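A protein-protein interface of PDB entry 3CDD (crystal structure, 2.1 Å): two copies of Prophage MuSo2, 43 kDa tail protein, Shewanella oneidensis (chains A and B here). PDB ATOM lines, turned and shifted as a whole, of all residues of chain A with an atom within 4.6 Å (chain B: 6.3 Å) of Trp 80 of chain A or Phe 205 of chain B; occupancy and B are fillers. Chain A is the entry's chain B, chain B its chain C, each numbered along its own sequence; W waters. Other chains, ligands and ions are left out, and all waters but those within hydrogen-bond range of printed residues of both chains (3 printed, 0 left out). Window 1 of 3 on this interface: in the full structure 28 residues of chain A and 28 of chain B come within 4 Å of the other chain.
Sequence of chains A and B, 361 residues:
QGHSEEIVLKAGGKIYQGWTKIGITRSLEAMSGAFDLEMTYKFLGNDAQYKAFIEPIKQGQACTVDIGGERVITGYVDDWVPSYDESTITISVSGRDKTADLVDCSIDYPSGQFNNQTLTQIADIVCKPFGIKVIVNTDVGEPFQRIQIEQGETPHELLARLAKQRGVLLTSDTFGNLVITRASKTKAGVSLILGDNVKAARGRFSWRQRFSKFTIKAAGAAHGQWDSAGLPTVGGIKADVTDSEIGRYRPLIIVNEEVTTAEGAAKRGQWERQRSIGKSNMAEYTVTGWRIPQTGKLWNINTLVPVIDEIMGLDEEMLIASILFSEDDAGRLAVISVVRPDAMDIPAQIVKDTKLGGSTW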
ATOM      1  N   PRO A  56      24.912  -4.216 -15.610  1.00  0.00           N
ATOM      2  CA  PRO A  56      24.601  -3.431 -14.413  1.00  0.00           C
ATOM      3  C   PRO A  56      25.192  -2.018 -14.437  1.00  0.00           C
ATOM      4  O   PRO A  56      26.371  -1.837 -14.766  1.00  0.00           O
ATOM      5  CB  PRO A  56      25.234  -4.257 -13.289  1.00  0.00           C
ATOM      6  CG  PRO A  56      25.186  -5.653 -13.799  1.00  0.00           C
ATOM      7  CD  PRO A  56      25.527  -5.511 -15.259  1.00  0.00           C
ATOM      8  N   ILE A  57      24.356  -1.033 -14.118  1.00  0.00           N
ATOM      9  CA  ILE A  57      24.783   0.355 -13.958  1.00  0.00           C
ATOM     10  C   ILE A  57      25.458   0.447 -12.588  1.00  0.00           C
ATOM     11  O   ILE A  57      24.818   0.177 -11.592  1.00  0.00           O
ATOM     12  CB  ILE A  57      23.566   1.338 -14.070  1.00  0.00           C
ATOM     13  CG1 ILE A  57      22.815   1.125 -15.404  1.00  0.00           C
ATOM     14  CG2 ILE A  57      24.023   2.798 -13.950  1.00  0.00           C
ATOM     15  CD1 ILE A  57      21.509   1.907 -15.581  1.00  0.00           C
ATOM     16  N   GLN A  59      26.783   1.827  -9.154  1.00  0.00           N
ATOM     17  CA  GLN A  59      26.567   2.911  -8.173  1.00  0.00           C
ATOM     18  C   GLN A  59      27.833   3.763  -7.962  1.00  0.00           C
ATOM     19  O   GLN A  59      28.955   3.257  -8.016  1.00  0.00           O
ATOM     20  CB  GLN A  59      26.076   2.353  -6.829  1.00  0.00           C
ATOM     21  CG  GLN A  59      27.077   1.443  -6.077  1.00  0.00           C
ATOM     22  CD  GLN A  59      27.141  -0.005  -6.576  1.00  0.00           C
ATOM     23  OE1 GLN A  59      26.512  -0.386  -7.569  1.00  0.00           O
ATOM     24  NE2 GLN A  59      27.921  -0.819  -5.880  1.00  0.00           N
ATOM     25  N   ASP A  78      23.488   7.079  -6.789  1.00  0.00           N
ATOM     26  CA  ASP A  78      23.603   6.567  -5.432  1.00  0.00           C
ATOM     27  C   ASP A  78      23.410   5.058  -5.399  1.00  0.00           C
ATOM     28  O   ASP A  78      24.208   4.356  -4.780  1.00  0.00           O
ATOM     29  CB  ASP A  78      22.532   7.182  -4.522  1.00  0.00           C
ATOM     30  CG  ASP A  78      22.805   8.605  -4.181  1.00  0.00           C
ATOM     31  OD1 ASP A  78      23.974   8.969  -3.961  1.00  0.00           O
ATOM     32  OD2 ASP A  78      21.842   9.379  -4.121  1.00  0.00           O
ATOM     33  N   ASP A  79      22.323   4.576  -6.020  1.00  0.00           N
ATOM     34  CA  ASP A  79      21.822   3.213  -5.813  1.00  0.00           C
ATOM     35  C   ASP A  79      21.645   2.438  -7.112  1.00  0.00           C
ATOM     36  O   ASP A  79      21.037   2.924  -8.076  1.00  0.00           O
ATOM     37  CB  ASP A  79      20.442   3.197  -5.132  1.00  0.00           C
ATOM     38  CG  ASP A  79      20.344   4.110  -3.901  1.00  0.00           C
ATOM     39  OD1 ASP A  79      21.122   3.950  -2.954  1.00  0.00           O
ATOM     40  OD2 ASP A  79      19.434   4.985  -3.872  1.00  0.00           O
ATOM     41  N   TRP A  80      22.125   1.203  -7.108  1.00  0.00           N
ATOM     42  CA  TRP A  80      21.797   0.252  -8.146  1.00  0.00           C
ATOM     43  C   TRP A  80      20.852  -0.777  -7.505  1.00  0.00           C
ATOM     44  O   TRP A  80      21.207  -1.414  -6.518  1.00  0.00           O
ATOM     45  CB  TRP A  80      23.089  -0.370  -8.698  1.00  0.00           C
ATOM     46  CG  TRP A  80      22.930  -1.651  -9.515  1.00  0.00           C
ATOM     47  CD1 TRP A  80      23.465  -2.869  -9.219  1.00  0.00           C
ATOM     48  CD2 TRP A  80      22.210  -1.822 -10.755  1.00  0.00           C
ATOM     49  NE1 TRP A  80      23.126  -3.780 -10.183  1.00  0.00           N
ATOM     50  CE2 TRP A  80      22.358  -3.171 -11.137  1.00  0.00           C
ATOM     51  CE3 TRP A  80      21.470  -0.961 -11.583  1.00  0.00           C
ATOM     52  CZ2 TRP A  80      21.787  -3.694 -12.310  1.00  0.00           C
ATOM     53  CZ3 TRP A  80      20.886  -1.484 -12.751  1.00  0.00           C
ATOM     54  CH2 TRP A  80      21.061  -2.841 -13.107  1.00  0.00           C
ATOM     55  N   VAL A  81      19.642  -0.878  -8.062  1.00  0.00           N
ATOM     56  CA  VAL A  81      18.544  -1.650  -7.507  1.00  0.00           C
ATOM     57  C   VAL A  81      17.933  -2.644  -8.529  1.00  0.00           C
ATOM     58  O   VAL A  81      16.863  -2.372  -9.137  1.00  0.00           O
ATOM     59  CB  VAL A  81      17.422  -0.706  -6.950  1.00  0.00           C
ATOM     60  CG1 VAL A  81      16.491  -1.451  -6.045  1.00  0.00           C
ATOM     61  CG2 VAL A  81      18.035   0.495  -6.204  1.00  0.00           C
ATOM     62  N   PRO A  82      18.590  -3.812  -8.704  1.00  0.00           N
ATOM     63  CA  PRO A  82      18.064  -4.856  -9.595  1.00  0.00           C
ATOM     64  C   PRO A  82      17.131  -5.853  -8.902  1.00  0.00           C
ATOM     65  O   PRO A  82      17.327  -6.175  -7.712  1.00  0.00           O
ATOM     66  CB  PRO A  82      19.326  -5.589 -10.014  1.00  0.00           C
ATOM     67  CG  PRO A  82      20.169  -5.555  -8.764  1.00  0.00           C
ATOM     68  CD  PRO A  82      19.852  -4.244  -8.066  1.00  0.00           C
ATOM     69  N   ILE A  91      15.050  -3.229 -13.314  1.00  0.00           N
ATOM     70  CA  ILE A  91      16.279  -2.549 -12.904  1.00  0.00           C
ATOM     71  C   ILE A  91      15.966  -1.108 -12.621  1.00  0.00           C
ATOM     72  O   ILE A  91      15.210  -0.475 -13.352  1.00  0.00           O
ATOM     73  CB  ILE A  91      17.455  -2.695 -13.914  1.00  0.00           C
ATOM     74  CG1 ILE A  91      17.175  -1.977 -15.251  1.00  0.00           C
ATOM     75  CG2 ILE A  91      17.800  -4.174 -14.113  1.00  0.00           C
ATOM     76  CD1 ILE A  91      17.734  -0.544 -15.353  1.00  0.00           C
ATOM     77  N   SER A  92      16.547  -0.599 -11.548  1.00  0.00           N
ATOM     78  CA  SER A  92      16.259   0.734 -11.123  1.00  0.00           C
ATOM     79  C   SER A  92      17.533   1.408 -10.617  1.00  0.00           C
ATOM     80  O   SER A  92      18.384   0.773  -9.985  1.00  0.00           O
ATOM     81  CB  SER A  92      15.196   0.677 -10.024  1.00  0.00           C
ATOM     82  OG  SER A  92      14.730   1.959  -9.694  1.00  0.00           O
ATOM     83  N   VAL A  93      17.668   2.693 -10.925  1.00  0.00           N
ATOM     84  CA  VAL A  93      18.752   3.509 -10.396  1.00  0.00           C
ATOM     85  C   VAL A  93      18.181   4.756  -9.756  1.00  0.00           C
ATOM     86  O   VAL A  93      17.155   5.294 -10.208  1.00  0.00           O
ATOM     87  CB  VAL A  93      19.859   3.874 -11.459  1.00  0.00           C
ATOM     88  CG1 VAL A  93      20.730   2.670 -11.768  1.00  0.00           C
ATOM     89  CG2 VAL A  93      19.264   4.488 -12.758  1.00  0.00           C
ATOM     90  N   ARG B 202      16.464  -9.905  -5.315  1.00  0.00           N
ATOM     91  CA  ARG B 202      16.191  -8.525  -4.985  1.00  0.00           C
ATOM     92  C   ARG B 202      17.547  -7.994  -4.525  1.00  0.00           C
ATOM     93  O   ARG B 202      18.257  -8.698  -3.807  1.00  0.00           O
ATOM     94  CB  ARG B 202      15.268  -8.571  -3.769  1.00  0.00           C
ATOM     95  CG  ARG B 202      14.541  -7.383  -3.394  1.00  0.00           C
ATOM     96  CD  ARG B 202      13.764  -7.715  -2.141  1.00  0.00           C
ATOM     97  NE  ARG B 202      13.371  -6.490  -1.481  1.00  0.00           N
ATOM     98  CZ  ARG B 202      13.520  -6.226  -0.190  1.00  0.00           C
ATOM     99  NH1 ARG B 202      14.027  -7.129   0.647  1.00  0.00           N
ATOM    100  NH2 ARG B 202      13.137  -5.041   0.261  1.00  0.00           N
ATOM    101  N   GLY B 203      17.911  -6.766  -4.900  1.00  0.00           N
ATOM    102  CA  GLY B 203      19.200  -6.232  -4.466  1.00  0.00           C
ATOM    103  C   GLY B 203      19.209  -4.721  -4.394  1.00  0.00           C
ATOM    104  O   GLY B 203      18.476  -4.071  -5.118  1.00  0.00           O
ATOM    105  N   ARG B 204      20.052  -4.166  -3.529  1.00  0.00           N
ATOM    106  CA  ARG B 204      20.258  -2.726  -3.476  1.00  0.00           C
ATOM    107  C   ARG B 204      21.724  -2.485  -3.122  1.00  0.00           C
ATOM    108  O   ARG B 204      22.210  -2.948  -2.089  1.00  0.00           O
ATOM    109  CB  ARG B 204      19.280  -2.077  -2.461  1.00  0.00           C
ATOM    110  CG  ARG B 204      19.495  -0.579  -2.162  1.00  0.00           C
ATOM    111  CD  ARG B 204      18.398  -0.056  -1.184  1.00  0.00           C
ATOM    112  NE  ARG B 204      17.080  -0.142  -1.829  1.00  0.00           N
ATOM    113  CZ  ARG B 204      16.548   0.802  -2.604  1.00  0.00           C
ATOM    114  NH1 ARG B 204      17.194   1.937  -2.814  1.00  0.00           N
ATOM    115  NH2 ARG B 204      15.360   0.611  -3.166  1.00  0.00           N
ATOM    116  N   PHE B 205      22.428  -1.781  -4.005  1.00  0.00           N
ATOM    117  CA  PHE B 205      23.854  -1.473  -3.844  1.00  0.00           C
ATOM    118  C   PHE B 205      24.028   0.031  -3.956  1.00  0.00           C
ATOM    119  O   PHE B 205      23.757   0.643  -5.007  1.00  0.00           O
ATOM    120  CB  PHE B 205      24.691  -2.236  -4.878  1.00  0.00           C
ATOM    121  CG  PHE B 205      24.306  -3.690  -5.000  1.00  0.00           C
ATOM    122  CD1 PHE B 205      24.915  -4.663  -4.187  1.00  0.00           C
ATOM    123  CD2 PHE B 205      23.313  -4.092  -5.905  1.00  0.00           C
ATOM    124  CE1 PHE B 205      24.538  -6.008  -4.280  1.00  0.00           C
ATOM    125  CE2 PHE B 205      22.935  -5.430  -6.014  1.00  0.00           C
ATOM    126  CZ  PHE B 205      23.538  -6.392  -5.203  1.00  0.00           C
ATOM    127  N   SER B 206      24.468   0.624  -2.854  1.00  0.00           N
ATOM    128  CA  SER B 206      24.407   2.054  -2.654  1.00  0.00           C
ATOM    129  C   SER B 206      25.775   2.652  -2.232  1.00  0.00           C
ATOM    130  O   SER B 206      26.630   1.952  -1.684  1.00  0.00           O
ATOM    131  CB  SER B 206      23.322   2.325  -1.602  1.00  0.00           C
ATOM    132  OG  SER B 206      23.060   3.704  -1.402  1.00  0.00           O
ATOM    133  N   TRP B 207      25.978   3.941  -2.510  1.00  0.00           N
ATOM    134  CA  TRP B 207      27.090   4.691  -1.939  1.00  0.00           C
ATOM    135  C   TRP B 207      26.634   5.766  -0.958  1.00  0.00           C
ATOM    136  O   TRP B 207      27.456   6.557  -0.507  1.00  0.00           O
ATOM    137  CB  TRP B 207      27.920   5.353  -3.032  1.00  0.00           C
ATOM    138  CG  TRP B 207      28.962   4.485  -3.668  1.00  0.00           C
ATOM    139  CD1 TRP B 207      29.003   3.115  -3.709  1.00  0.00           C
ATOM    140  CD2 TRP B 207      30.103   4.943  -4.394  1.00  0.00           C
ATOM    141  NE1 TRP B 207      30.126   2.697  -4.404  1.00  0.00           N
ATOM    142  CE2 TRP B 207      30.807   3.801  -4.841  1.00  0.00           C
ATOM    143  CE3 TRP B 207      30.600   6.212  -4.717  1.00  0.00           C
ATOM    144  CZ2 TRP B 207      31.973   3.897  -5.589  1.00  0.00           C
ATOM    145  CZ3 TRP B 207      31.747   6.303  -5.456  1.00  0.00           C
ATOM    146  CH2 TRP B 207      32.427   5.154  -5.881  1.00  0.00           C
ATOM    147  N   SER B 280      25.583  -0.883   3.096  1.00  0.00           N
ATOM    148  CA  SER B 280      25.384  -0.308   1.768  1.00  0.00           C
ATOM    149  C   SER B 280      25.025  -1.318   0.677  1.00  0.00           C
ATOM    150  O   SER B 280      24.628  -0.923  -0.424  1.00  0.00           O
ATOM    151  CB  SER B 280      26.640   0.454   1.352  1.00  0.00           C
ATOM    152  OG  SER B 280      26.856   1.551   2.227  1.00  0.00           O
ATOM    153  N   ASN B 281      25.189  -2.604   0.969  1.00  0.00           N
ATOM    154  CA  ASN B 281      24.816  -3.639   0.023  1.00  0.00           C
ATOM    155  C   ASN B 281      23.760  -4.569   0.608  1.00  0.00           C
ATOM    156  O   ASN B 281      23.829  -4.934   1.792  1.00  0.00           O
ATOM    157  CB  ASN B 281      26.029  -4.444  -0.425  1.00  0.00           C
ATOM    158  CG  ASN B 281      27.108  -3.585  -1.041  1.00  0.00           C
ATOM    159  OD1 ASN B 281      26.830  -2.614  -1.747  1.00  0.00           O
ATOM    160  ND2 ASN B 281      28.359  -3.943  -0.783  1.00  0.00           N
ATOM    161  N   MET B 282      22.775  -4.910  -0.218  1.00  0.00           N
ATOM    162  CA  MET B 282      21.789  -5.934   0.099  1.00  0.00           C
ATOM    163  C   MET B 282      21.684  -6.887  -1.094  1.00  0.00           C
ATOM    164  O   MET B 282      21.703  -6.454  -2.241  1.00  0.00           O
ATOM    165  CB  MET B 282      20.415  -5.307   0.397  1.00  0.00           C
ATOM    166  CG  MET B 282      19.249  -6.319   0.334  1.00  0.00           C
ATOM    167  SD  MET B 282      17.481  -5.522   0.254  1.00  0.00           S
ATOM    168  CE  MET B 282      17.086  -5.971  -1.575  1.00  0.00           C
ATOM    169  N   ALA B 283      21.584  -8.183  -0.813  1.00  0.00           N
ATOM    170  CA  ALA B 283      21.242  -9.177  -1.852  1.00  0.00           C
ATOM    171  C   ALA B 283      20.437 -10.300  -1.204  1.00  0.00           C
ATOM    172  O   ALA B 283      20.897 -10.940  -0.283  1.00  0.00           O
ATOM    173  CB  ALA B 283      22.465  -9.701  -2.530  1.00  0.00           C
ATOM    174  N   GLU B 310      24.109 -12.416 -13.399  1.00  0.00           N
ATOM    175  CA  GLU B 310      24.335 -11.344 -14.377  1.00  0.00           C
ATOM    176  C   GLU B 310      23.371 -10.169 -14.247  1.00  0.00           C
ATOM    177  O   GLU B 310      23.706  -9.046 -14.610  1.00  0.00           O
ATOM    178  CB  GLU B 310      24.217 -11.883 -15.805  1.00  0.00           C
ATOM    179  CG  GLU B 310      25.460 -12.517 -16.370  1.00  0.00           C
ATOM    180  CD  GLU B 310      25.215 -13.130 -17.734  1.00  0.00           C
ATOM    181  OE1 GLU B 310      26.192 -13.612 -18.361  1.00  0.00           O
ATOM    182  OE2 GLU B 310      24.041 -13.131 -18.177  1.00  0.00           O
ATOM    183  N   ILE B 311      22.161 -10.421 -13.768  1.00  0.00           N
ATOM    184  CA  ILE B 311      21.195  -9.317 -13.617  1.00  0.00           C
ATOM    185  C   ILE B 311      21.703  -8.302 -12.579  1.00  0.00           C
ATOM    186  O   ILE B 311      21.826  -7.099 -12.876  1.00  0.00           O
ATOM    187  CB  ILE B 311      19.746  -9.825 -13.343  1.00  0.00           C
ATOM    188  CG1 ILE B 311      19.212 -10.549 -14.578  1.00  0.00           C
ATOM    189  CG2 ILE B 311      18.760  -8.639 -12.993  1.00  0.00           C
ATOM    190  CD1 ILE B 311      18.063 -11.484 -14.303  1.00  0.00           C
ATOM    191  N   MET B 312      22.043  -8.797 -11.389  1.00  0.00           N
ATOM    192  CA  MET B 312      22.612  -7.943 -10.322  1.00  0.00           C
ATOM    193  C   MET B 312      24.038  -7.524 -10.563  1.00  0.00           C
ATOM    194  O   MET B 312      24.416  -6.412 -10.195  1.00  0.00           O
ATOM    195  CB  MET B 312      22.570  -8.643  -8.986  1.00  0.00           C
ATOM    196  CG  MET B 312      21.209  -9.130  -8.668  1.00  0.00           C
ATOM    197  SD  MET B 312      20.809  -8.937  -6.788  1.00  0.00           S
ATOM    198  CE  MET B 312      19.015  -9.225  -7.009  1.00  0.00           C
ATOM    199  N   GLY B 313      24.821  -8.420 -11.169  1.00  0.00           N
ATOM    200  CA  GLY B 313      26.249  -8.203 -11.370  1.00  0.00           C
ATOM    201  C   GLY B 313      27.033  -8.846 -10.242  1.00  0.00           C
ATOM    202  O   GLY B 313      27.962  -8.246  -9.711  1.00  0.00           O
ATOM    203  N   LEU B 314      26.647 -10.062  -9.870  1.00  0.00           N
ATOM    204  CA  LEU B 314      27.343 -10.804  -8.838  1.00  0.00           C
ATOM    205  C   LEU B 314      27.937 -12.081  -9.393  1.00  0.00           C
ATOM    206  O   LEU B 314      27.230 -12.895  -9.998  1.00  0.00           O
ATOM    207  CB  LEU B 314      26.422 -11.127  -7.655  1.00  0.00           C
ATOM    208  CG  LEU B 314      25.946  -9.946  -6.799  1.00  0.00           C
ATOM    209  CD1 LEU B 314      25.052 -10.468  -5.690  1.00  0.00           C
ATOM    210  CD2 LEU B 314      27.134  -9.142  -6.219  1.00  0.00           C
HETATM  211  O   HOH W   1      16.653   4.083  -4.687  1.00  0.00           O
HETATM  212  O   HOH W   2      26.597   8.522  -2.718  1.00  0.00           O
HETATM  213  O   HOH W   3      19.858   3.213  -0.314  1.00  0.00           O
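Trp 80 of chain A touches just these residues of chain B: Arg 204, Phe 205, Ile 311 and Met 312. Phe 205 of chain B touches just these residues of chain A: Gln 59, Asp 78, Asp 79, Trp 80 and Pro 82. Of the printed residues of chain B, Asp 78 of chain A touches Phe 205, Ser 206 and Trp 207. Printed residues of chain A within 4 Å of Ile 311 of chain B: Pro 56 and Trp 80. Of the printed residues of chain B, Pro 82 of chain A touches Arg 202 (3.7 Å), Gly 203 (2.9 Å), Phe 205 (3.9 Å) and Met 312 (3.6 Å). Of the printed residues of chain A, Trp 207 of chain B touches Gln 59 and Asp 78. Of the printed residues of chain B, Gln 59 of chain A touches Phe 205 (3.4 Å) and Trp 207 (3.5 Å). Ile 57 of chain A touches none of the printed residues of chain B.
Water W1 lies within hydrogen-bond range of the guanidinium group (NH1) of Arg 204 of chain B (2.9 Å) and the side-chain carboxylate (OD2) of Asp 79 of chain A (3.0 Å). Water W2 lies within hydrogen-bond range of OD1 of Asp 78 of chain A (2.9 Å) and O of Trp 207 of chain B (3.1 Å). Water W3 lies within hydrogen-bond range of the side-chain carboxylate of Asp 79 of chain A and the side-chain hydroxyl of Ser 206 of chain B.
Among the printed residues, merely in contact across the chains: Pro 56 of chain A with Glu 310 of chain B (3.8 Å), Pro 56 of chain A with Ile 311 of chain B (3.8 Å), Pro 56 of chain A with Met 312 of chain B (3.8 Å), Pro 56 of chain A with Gly 313 of chain B (3.7 Å), Gln 59 of chain A with Phe 205 of chain B (3.4 Å), Gln 59 of chain A with Trp 207 of chain B (3.5 Å), Asp 78 of chain A with Phe 205 of chain B (3.7 Å), Asp 78 of chain A with Ser 206 of chain B (3.1 Å), Asp 79 of chain A with Phe 205 of chain B (3.3 Å), Trp 80 of chain A with Arg 204 of chain B (3.4 Å), Trp 80 of chain A with Ile 311 of chain B (3.5 Å), Val 81 of chain A with Gly 203 of chain B (3.4 Å), Val 81 of chain A with Arg 204 of chain B (3.7 Å), Pro 82 of chain A with Arg 202 of chain B (3.7 Å), Pro 82 of chain A with Phe 205 of chain B (3.9 Å) and Pro 82 of chain A with Met 312 of chain B (3.6 Å).
No position is printed for both chains.
The backbone carbonyl oxygen (O) of Asp 78 of chain A sits at hydrogen-bond distance from the backbone NH (N) of Trp 207 of chain B, at 2.9 Å. The side-chain carboxylate (OD2) of Asp 79 of chain A is in salt-bridge range of the guanidinium group (NH1) of Arg 204 of chain B (3.9 Å). OD1 of Asp 79 of chain A lies within hydrogen-bond range of OG of Ser 206 of chain B. The backbone carbonyl oxygen of Phe 205 of chain B lies within hydrogen-bond range of the backbone NH of Trp 80 of chain A (2.7 Å). NE1 of Trp 80 of chain A lies within hydrogen-bond range of O of Met 312 of chain B, 2.9 Å away. The backbone carbonyl oxygen (O) of Pro 82 of chain A sits at hydrogen-bond distance from the backbone NH (N) of Gly 203 of chain B, at 2.9 Å.
The backbone carbonyl oxygen of Ser 92 of chain A sits at hydrogen-bond distance from the backbone NH of Val 81 of chain A, 2.8 Å away. N of Met 282 of chain B lies within hydrogen-bond range of O of Arg 204 of chain B, 2.8 Å away. The backbone NH (N) of Ser 206 of chain B sits at hydrogen-bond distance from the backbone carbonyl oxygen (O) of Ser 280 of chain B.
Of the 11 printed residues of chain A, 7 touch a printed residue of chain B. Hydrophobic or aromatic side chains of chain A that line the printed part of chain B: Pro 56, Trp 80, Val 81 and Pro 82. Printed residues of chain B that touch a printed residue of chain A: Arg 202, Gly 203, Arg 204, Phe 205, Ser 206, Trp 207, Glu 310, Ile 311, Met 312 and Gly 313. Hydrophobic or aromatic side chains of chain B that line the printed part of chain A: Phe 205, Trp 207 and Met 312. Among the printed residues, Asp or Glu carboxylates within 4 Å of a Lys or Arg side-chain nitrogen of the other chain: Asp 79 of chain A with Arg 204 of chain B (3.9 Å).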
